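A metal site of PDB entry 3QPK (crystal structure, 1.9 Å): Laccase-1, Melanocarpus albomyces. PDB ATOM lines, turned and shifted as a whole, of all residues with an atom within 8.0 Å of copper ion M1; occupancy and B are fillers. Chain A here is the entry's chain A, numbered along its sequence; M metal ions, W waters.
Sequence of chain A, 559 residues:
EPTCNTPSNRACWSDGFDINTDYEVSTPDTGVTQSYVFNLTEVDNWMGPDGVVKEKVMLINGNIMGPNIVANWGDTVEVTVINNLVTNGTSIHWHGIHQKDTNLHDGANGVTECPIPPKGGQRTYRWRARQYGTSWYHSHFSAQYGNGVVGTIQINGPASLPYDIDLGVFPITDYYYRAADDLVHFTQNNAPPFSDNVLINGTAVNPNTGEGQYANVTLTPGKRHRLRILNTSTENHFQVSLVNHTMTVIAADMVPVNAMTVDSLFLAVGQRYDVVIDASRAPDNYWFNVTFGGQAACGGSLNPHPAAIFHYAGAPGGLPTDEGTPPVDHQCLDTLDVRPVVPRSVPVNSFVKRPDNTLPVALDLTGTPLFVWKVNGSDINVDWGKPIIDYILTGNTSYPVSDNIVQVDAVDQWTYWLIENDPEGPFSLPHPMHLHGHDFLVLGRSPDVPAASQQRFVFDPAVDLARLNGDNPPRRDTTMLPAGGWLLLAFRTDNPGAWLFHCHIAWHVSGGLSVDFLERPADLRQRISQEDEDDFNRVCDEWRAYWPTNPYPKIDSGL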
ATOM      1  N   HIS A  93      21.019 -13.510 -15.553  1.00  0.00           N
ATOM      2  CA  HIS A  93      20.594 -12.125 -15.600  1.00  0.00           C
ATOM      3  C   HIS A  93      19.643 -11.907 -16.771  1.00  0.00           C
ATOM      4  O   HIS A  93      19.841 -12.430 -17.868  1.00  0.00           O
ATOM      5  CB  HIS A  93      21.823 -11.195 -15.646  1.00  0.00           C
ATOM      6  CG  HIS A  93      21.519  -9.764 -15.937  1.00  0.00           C
ATOM      7  ND1 HIS A  93      20.749  -8.987 -15.103  1.00  0.00           N
ATOM      8  CD2 HIS A  93      21.890  -8.949 -16.955  1.00  0.00           C
ATOM      9  CE1 HIS A  93      20.634  -7.770 -15.600  1.00  0.00           C
ATOM     10  NE2 HIS A  93      21.318  -7.721 -16.726  1.00  0.00           N
ATOM     11  N   TRP A  94      18.579 -11.170 -16.509  1.00  0.00           N
ATOM     12  CA  TRP A  94      17.569 -10.864 -17.501  1.00  0.00           C
ATOM     13  C   TRP A  94      17.845  -9.478 -18.067  1.00  0.00           C
ATOM     14  O   TRP A  94      17.352  -8.471 -17.542  1.00  0.00           O
ATOM     15  CB  TRP A  94      16.189 -10.967 -16.835  1.00  0.00           C
ATOM     16  CG  TRP A  94      16.142 -12.204 -15.949  1.00  0.00           C
ATOM     17  CD1 TRP A  94      16.360 -12.268 -14.605  1.00  0.00           C
ATOM     18  CD2 TRP A  94      15.909 -13.544 -16.380  1.00  0.00           C
ATOM     19  NE1 TRP A  94      16.261 -13.576 -14.170  1.00  0.00           N
ATOM     20  CE2 TRP A  94      15.983 -14.379 -15.246  1.00  0.00           C
ATOM     21  CE3 TRP A  94      15.646 -14.132 -17.633  1.00  0.00           C
ATOM     22  CZ2 TRP A  94      15.802 -15.762 -15.314  1.00  0.00           C
ATOM     23  CZ3 TRP A  94      15.462 -15.485 -17.695  1.00  0.00           C
ATOM     24  CH2 TRP A  94      15.547 -16.291 -16.550  1.00  0.00           C
ATOM     25  N   HIS A  95      18.656  -9.423 -19.115  1.00  0.00           N
ATOM     26  CA  HIS A  95      19.173  -8.160 -19.658  1.00  0.00           C
ATOM     27  C   HIS A  95      18.078  -7.304 -20.289  1.00  0.00           C
ATOM     28  O   HIS A  95      17.477  -7.693 -21.294  1.00  0.00           O
ATOM     29  CB  HIS A  95      20.277  -8.441 -20.675  1.00  0.00           C
ATOM     30  CG  HIS A  95      20.867  -7.217 -21.291  1.00  0.00           C
ATOM     31  ND1 HIS A  95      22.222  -6.965 -21.282  1.00  0.00           N
ATOM     32  CD2 HIS A  95      20.290  -6.178 -21.949  1.00  0.00           C
ATOM     33  CE1 HIS A  95      22.450  -5.809 -21.902  1.00  0.00           C
ATOM     34  NE2 HIS A  95      21.292  -5.315 -22.316  1.00  0.00           N
ATOM     35  N   GLY A  96      17.821  -6.138 -19.718  1.00  0.00           N
ATOM     36  CA  GLY A  96      16.772  -5.263 -20.221  1.00  0.00           C
ATOM     37  C   GLY A  96      15.551  -5.236 -19.325  1.00  0.00           C
ATOM     38  O   GLY A  96      14.708  -4.346 -19.420  1.00  0.00           O
ATOM     39  N   TRP A 136      17.070 -10.098 -23.672  1.00  0.00           N
ATOM     40  CA  TRP A 136      17.765 -11.370 -23.640  1.00  0.00           C
ATOM     41  C   TRP A 136      18.224 -11.660 -22.230  1.00  0.00           C
ATOM     42  O   TRP A 136      18.204 -10.801 -21.365  1.00  0.00           O
ATOM     43  CB  TRP A 136      18.960 -11.406 -24.605  1.00  0.00           C
ATOM     44  CG  TRP A 136      20.078 -10.414 -24.326  1.00  0.00           C
ATOM     45  CD1 TRP A 136      19.954  -9.049 -24.182  1.00  0.00           C
ATOM     46  CD2 TRP A 136      21.491 -10.691 -24.222  1.00  0.00           C
ATOM     47  NE1 TRP A 136      21.202  -8.478 -23.988  1.00  0.00           N
ATOM     48  CE2 TRP A 136      22.154  -9.465 -24.009  1.00  0.00           C
ATOM     49  CE3 TRP A 136      22.250 -11.869 -24.309  1.00  0.00           C
ATOM     50  CZ2 TRP A 136      23.540  -9.372 -23.866  1.00  0.00           C
ATOM     51  CZ3 TRP A 136      23.636 -11.776 -24.166  1.00  0.00           C
ATOM     52  CH2 TRP A 136      24.257 -10.537 -23.938  1.00  0.00           C
ATOM     53  N   TYR A 137      18.633 -12.900 -22.008  1.00  0.00           N
ATOM     54  CA  TYR A 137      19.097 -13.321 -20.704  1.00  0.00           C
ATOM     55  C   TYR A 137      20.413 -14.053 -20.870  1.00  0.00           C
ATOM     56  O   TYR A 137      20.696 -14.601 -21.951  1.00  0.00           O
ATOM     57  CB  TYR A 137      18.035 -14.202 -19.997  1.00  0.00           C
ATOM     58  CG  TYR A 137      17.692 -15.485 -20.742  1.00  0.00           C
ATOM     59  CD1 TYR A 137      18.456 -16.634 -20.580  1.00  0.00           C
ATOM     60  CD2 TYR A 137      16.605 -15.545 -21.602  1.00  0.00           C
ATOM     61  CE1 TYR A 137      18.149 -17.804 -21.259  1.00  0.00           C
ATOM     62  CE2 TYR A 137      16.277 -16.705 -22.291  1.00  0.00           C
ATOM     63  CZ  TYR A 137      17.067 -17.833 -22.118  1.00  0.00           C
ATOM     64  OH  TYR A 137      16.748 -19.008 -22.778  1.00  0.00           O
ATOM     65  N   HIS A 138      21.221 -14.071 -19.829  1.00  0.00           N
ATOM     66  CA  HIS A 138      22.507 -14.741 -19.921  1.00  0.00           C
ATOM     67  C   HIS A 138      23.107 -14.944 -18.558  1.00  0.00           C
ATOM     68  O   HIS A 138      22.722 -14.285 -17.611  1.00  0.00           O
ATOM     69  CB  HIS A 138      23.463 -13.916 -20.796  1.00  0.00           C
ATOM     70  CG  HIS A 138      23.659 -12.507 -20.320  1.00  0.00           C
ATOM     71  ND1 HIS A 138      24.551 -12.179 -19.323  1.00  0.00           N
ATOM     72  CD2 HIS A 138      23.083 -11.348 -20.724  1.00  0.00           C
ATOM     73  CE1 HIS A 138      24.509 -10.869 -19.120  1.00  0.00           C
ATOM     74  NE2 HIS A 138      23.623 -10.349 -19.953  1.00  0.00           N
ATOM     75  N   SER A 139      24.042 -15.879 -18.444  1.00  0.00           N
ATOM     76  CA  SER A 139      24.794 -16.058 -17.217  1.00  0.00           C
ATOM     77  C   SER A 139      25.571 -14.810 -16.857  1.00  0.00           C
ATOM     78  O   SER A 139      26.054 -14.066 -17.730  1.00  0.00           O
ATOM     79  CB  SER A 139      25.759 -17.238 -17.334  1.00  0.00           C
ATOM     80  OG  SER A 139      26.586 -17.329 -16.187  1.00  0.00           O
ATOM     81  N   HIS A 140      25.689 -14.578 -15.549  1.00  0.00           N
ATOM     82  CA  HIS A 140      26.540 -13.518 -15.051  1.00  0.00           C
ATOM     83  C   HIS A 140      27.684 -14.122 -14.233  1.00  0.00           C
ATOM     84  O   HIS A 140      28.297 -13.429 -13.436  1.00  0.00           O
ATOM     85  CB  HIS A 140      25.744 -12.490 -14.246  1.00  0.00           C
ATOM     86  CG  HIS A 140      26.040 -11.077 -14.643  1.00  0.00           C
ATOM     87  ND1 HIS A 140      27.277 -10.488 -14.439  1.00  0.00           N
ATOM     88  CD2 HIS A 140      25.275 -10.132 -15.236  1.00  0.00           C
ATOM     89  CE1 HIS A 140      27.243  -9.243 -14.886  1.00  0.00           C
ATOM     90  NE2 HIS A 140      26.043  -9.004 -15.373  1.00  0.00           N
ATOM     91  N   TYR A 145      28.592 -16.986 -20.024  1.00  0.00           N
ATOM     92  CA  TYR A 145      27.648 -16.923 -21.140  1.00  0.00           C
ATOM     93  C   TYR A 145      28.334 -17.111 -22.504  1.00  0.00           C
ATOM     94  O   TYR A 145      27.687 -17.481 -23.478  1.00  0.00           O
ATOM     95  CB  TYR A 145      26.763 -15.662 -21.118  1.00  0.00           C
ATOM     96  CG  TYR A 145      27.267 -14.346 -21.726  1.00  0.00           C
ATOM     97  CD1 TYR A 145      27.039 -14.036 -23.073  1.00  0.00           C
ATOM     98  CD2 TYR A 145      27.846 -13.368 -20.935  1.00  0.00           C
ATOM     99  CE1 TYR A 145      27.429 -12.805 -23.625  1.00  0.00           C
ATOM    100  CE2 TYR A 145      28.272 -12.134 -21.485  1.00  0.00           C
ATOM    101  CZ  TYR A 145      28.045 -11.866 -22.827  1.00  0.00           C
ATOM    102  OH  TYR A 145      28.451 -10.649 -23.357  1.00  0.00           O
ATOM    103  N   ASN A 231      22.295  -8.190 -30.417  1.00  0.00           N
ATOM    104  CA  ASN A 231      23.721  -8.519 -30.352  1.00  0.00           C
ATOM    105  C   ASN A 231      24.031  -9.196 -29.029  1.00  0.00           C
ATOM    106  O   ASN A 231      24.193  -8.541 -27.988  1.00  0.00           O
ATOM    107  CB  ASN A 231      24.605  -7.260 -30.562  1.00  0.00           C
ATOM    108  CG  ASN A 231      26.087  -7.586 -30.625  1.00  0.00           C
ATOM    109  OD1 ASN A 231      26.494  -8.726 -30.388  1.00  0.00           O
ATOM    110  ND2 ASN A 231      26.895  -6.588 -30.948  1.00  0.00           N
ATOM    111  N   THR A 232      24.107 -10.520 -29.055  1.00  0.00           N
ATOM    112  CA  THR A 232      24.306 -11.260 -27.828  1.00  0.00           C
ATOM    113  C   THR A 232      25.755 -11.680 -27.615  1.00  0.00           C
ATOM    114  O   THR A 232      26.012 -12.668 -26.921  1.00  0.00           O
ATOM    115  CB  THR A 232      23.388 -12.504 -27.795  1.00  0.00           C
ATOM    116  OG1 THR A 232      23.705 -13.326 -28.927  1.00  0.00           O
ATOM    117  CG2 THR A 232      21.925 -12.095 -27.872  1.00  0.00           C
ATOM    118  N   SER A 233      26.700 -10.937 -28.213  1.00  0.00           N
ATOM    119  CA  SER A 233      28.111 -11.324 -28.219  1.00  0.00           C
ATOM    120  C   SER A 233      28.797 -11.146 -26.861  1.00  0.00           C
ATOM    121  O   SER A 233      28.221 -10.571 -25.953  1.00  0.00           O
ATOM    122  CB  SER A 233      28.892 -10.497 -29.235  1.00  0.00           C
ATOM    123  OG  SER A 233      28.340 -10.601 -30.533  1.00  0.00           O
ATOM    124  N   VAL A 269      27.465  -4.558 -28.044  1.00  0.00           N
ATOM    125  CA  VAL A 269      27.160  -5.761 -27.291  1.00  0.00           C
ATOM    126  C   VAL A 269      25.987  -5.494 -26.339  1.00  0.00           C
ATOM    127  O   VAL A 269      26.020  -4.550 -25.553  1.00  0.00           O
ATOM    128  CB  VAL A 269      28.372  -6.208 -26.454  1.00  0.00           C
ATOM    129  CG1 VAL A 269      28.005  -7.403 -25.580  1.00  0.00           C
ATOM    130  CG2 VAL A 269      29.553  -6.518 -27.347  1.00  0.00           C
ATOM    131  N   GLY A 270      24.959  -6.338 -26.402  1.00  0.00           N
ATOM    132  CA  GLY A 270      23.798  -6.217 -25.527  1.00  0.00           C
ATOM    133  C   GLY A 270      22.680  -5.366 -26.099  1.00  0.00           C
ATOM    134  O   GLY A 270      21.552  -5.382 -25.572  1.00  0.00           O
ATOM    135  N   GLN A 271      22.989  -4.602 -27.146  1.00  0.00           N
ATOM    136  CA  GLN A 271      21.969  -3.783 -27.805  1.00  0.00           C
ATOM    137  C   GLN A 271      20.988  -4.604 -28.660  1.00  0.00           C
ATOM    138  O   GLN A 271      21.328  -5.654 -29.204  1.00  0.00           O
ATOM    139  CB  GLN A 271      22.593  -2.636 -28.619  1.00  0.00           C
ATOM    140  CG  GLN A 271      23.142  -1.487 -27.772  1.00  0.00           C
ATOM    141  CD  GLN A 271      23.515  -0.226 -28.569  1.00  0.00           C
ATOM    142  OE1 GLN A 271      23.988  -0.300 -29.703  1.00  0.00           O
ATOM    143  NE2 GLN A 271      23.333   0.937 -27.949  1.00  0.00           N
ATOM    144  N   ARG A 272      19.770  -4.074 -28.795  1.00  0.00           N
ATOM    145  CA  ARG A 272      18.736  -4.659 -29.628  1.00  0.00           C
ATOM    146  C   ARG A 272      18.079  -3.558 -30.463  1.00  0.00           C
ATOM    147  O   ARG A 272      18.040  -2.398 -30.048  1.00  0.00           O
ATOM    148  CB  ARG A 272      17.671  -5.367 -28.774  1.00  0.00           C
ATOM    149  CG  ARG A 272      18.152  -6.637 -28.047  1.00  0.00           C
ATOM    150  CD  ARG A 272      18.701  -6.309 -26.643  1.00  0.00           C
ATOM    151  NE  ARG A 272      17.657  -5.761 -25.785  1.00  0.00           N
ATOM    152  CZ  ARG A 272      17.866  -4.907 -24.789  1.00  0.00           C
ATOM    153  NH1 ARG A 272      19.098  -4.479 -24.514  1.00  0.00           N
ATOM    154  NH2 ARG A 272      16.837  -4.475 -24.053  1.00  0.00           N
ATOM    155  N   HIS A 434      26.555  -0.603 -19.844  1.00  0.00           N
ATOM    156  CA  HIS A 434      25.233  -1.176 -19.592  1.00  0.00           C
ATOM    157  C   HIS A 434      24.812  -0.978 -18.151  1.00  0.00           C
ATOM    158  O   HIS A 434      25.585  -1.261 -17.237  1.00  0.00           O
ATOM    159  CB  HIS A 434      25.208  -2.680 -19.928  1.00  0.00           C
ATOM    160  CG  HIS A 434      23.946  -3.368 -19.494  1.00  0.00           C
ATOM    161  ND1 HIS A 434      22.716  -3.090 -20.039  1.00  0.00           N
ATOM    162  CD2 HIS A 434      23.731  -4.317 -18.544  1.00  0.00           C
ATOM    163  CE1 HIS A 434      21.797  -3.827 -19.455  1.00  0.00           C
ATOM    164  NE2 HIS A 434      22.386  -4.582 -18.538  1.00  0.00           N
ATOM    165  N   HIS A 436      22.133  -1.954 -15.090  1.00  0.00           N
ATOM    166  CA  HIS A 436      21.069  -2.836 -14.570  1.00  0.00           C
ATOM    167  C   HIS A 436      20.016  -1.991 -13.897  1.00  0.00           C
ATOM    168  O   HIS A 436      20.337  -0.922 -13.360  1.00  0.00           O
ATOM    169  CB  HIS A 436      21.639  -3.787 -13.518  1.00  0.00           C
ATOM    170  CG  HIS A 436      22.520  -4.875 -14.054  1.00  0.00           C
ATOM    171  ND1 HIS A 436      22.433  -6.178 -13.637  1.00  0.00           N
ATOM    172  CD2 HIS A 436      23.507  -4.847 -14.989  1.00  0.00           C
ATOM    173  CE1 HIS A 436      23.326  -6.912 -14.279  1.00  0.00           C
ATOM    174  NE2 HIS A 436      23.987  -6.128 -15.112  1.00  0.00           N
ATOM    175  N   ASP A 477      19.251   0.807 -22.398  1.00  0.00           N
ATOM    176  CA  ASP A 477      20.028   0.181 -21.326  1.00  0.00           C
ATOM    177  C   ASP A 477      21.524   0.003 -21.634  1.00  0.00           C
ATOM    178  O   ASP A 477      22.322  -0.312 -20.751  1.00  0.00           O
ATOM    179  CB  ASP A 477      19.362  -1.122 -20.854  1.00  0.00           C
ATOM    180  CG  ASP A 477      19.352  -2.207 -21.923  1.00  0.00           C
ATOM    181  OD1 ASP A 477      20.422  -2.521 -22.478  1.00  0.00           O
ATOM    182  OD2 ASP A 477      18.264  -2.754 -22.198  1.00  0.00           O
ATOM    183  N   THR A 478      21.876   0.252 -22.894  1.00  0.00           N
ATOM    184  CA  THR A 478      23.251   0.100 -23.383  1.00  0.00           C
ATOM    185  C   THR A 478      23.576   1.206 -24.388  1.00  0.00           C
ATOM    186  O   THR A 478      22.780   1.487 -25.301  1.00  0.00           O
ATOM    187  CB  THR A 478      23.447  -1.293 -24.071  1.00  0.00           C
ATOM    188  OG1 THR A 478      23.232  -2.327 -23.110  1.00  0.00           O
ATOM    189  CG2 THR A 478      24.858  -1.424 -24.591  1.00  0.00           C
ATOM    190  N   HIS A 502      28.416  -1.420 -15.956  1.00  0.00           N
ATOM    191  CA  HIS A 502      29.673  -1.979 -16.425  1.00  0.00           C
ATOM    192  C   HIS A 502      29.764  -2.051 -17.942  1.00  0.00           C
ATOM    193  O   HIS A 502      28.764  -1.931 -18.639  1.00  0.00           O
ATOM    194  CB  HIS A 502      29.854  -3.368 -15.818  1.00  0.00           C
ATOM    195  CG  HIS A 502      28.858  -4.374 -16.302  1.00  0.00           C
ATOM    196  ND1 HIS A 502      29.063  -5.161 -17.409  1.00  0.00           N
ATOM    197  CD2 HIS A 502      27.646  -4.730 -15.812  1.00  0.00           C
ATOM    198  CE1 HIS A 502      28.023  -5.959 -17.598  1.00  0.00           C
ATOM    199  NE2 HIS A 502      27.142  -5.724 -16.640  1.00  0.00           N
ATOM    200  N   HIS A 504      30.022  -4.171 -21.219  1.00  0.00           N
ATOM    201  CA  HIS A 504      29.425  -5.489 -21.498  1.00  0.00           C
ATOM    202  C   HIS A 504      30.320  -6.435 -22.303  1.00  0.00           C
ATOM    203  O   HIS A 504      29.881  -7.533 -22.668  1.00  0.00           O
ATOM    204  CB  HIS A 504      28.079  -5.349 -22.218  1.00  0.00           C
ATOM    205  CG  HIS A 504      27.121  -6.471 -21.918  1.00  0.00           C
ATOM    206  ND1 HIS A 504      27.293  -7.748 -22.396  1.00  0.00           N
ATOM    207  CD2 HIS A 504      25.988  -6.493 -21.177  1.00  0.00           C
ATOM    208  CE1 HIS A 504      26.305  -8.511 -21.964  1.00  0.00           C
ATOM    209  NE2 HIS A 504      25.507  -7.769 -21.213  1.00  0.00           N
HETATM  210 CU    CU M   1      23.654  -8.369 -20.526  1.00  0.00          CU
HETATM  211 CU    CU M   2      21.883  -6.242 -17.676  1.00  0.00          CU
HETATM  212 CU    CU M   3      25.519  -7.099 -16.106  1.00  0.00          CU
HETATM  213  O   HOH W   1      24.623  -7.731 -18.220  1.00  0.00           O
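Copper ion M1 is bound by NE2 of His 138 (2.1 Å), NE2 of His 504 (2.1 Å), ND1 of His 95 (2.1 Å) and water W1 (2.6 Å).
O of His 138 lies within hydrogen-bond range of N of His 93 (2.8 Å). A ring nitrogen (ND1) of His 504 is in hydrogen-bond range of the side-chain hydroxyl of Tyr 145. N of His 95 lies within hydrogen-bond range of O of Trp 136, at 2.7 Å. A ring nitrogen (NE2) of His 95 lies close to a ring nitrogen (ND1) of His 434 (3.5 Å). O of Gly 270 is in hydrogen-bond range of NE2 of His 95. A ring nitrogen (NE2) of His 95 is in hydrogen-bond range of the side-chain carboxylate (OD1) of Asp 477 (2.9 Å). A ring nitrogen (NE2) of His 95 is in hydrogen-bond range of the guanidinium group (NH1) of Arg 272. The indole nitrogen (NE1) of Trp 136 is in hydrogen-bond range of the backbone carbonyl oxygen (O) of Gly 270 (3.5 Å).
Merely in contact with copper ion M1: Trp 136 (3.5 Å). Four residues have an atom within 4 Å of copper ion M1: His 95, Trp 136, His 138 and His 504.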
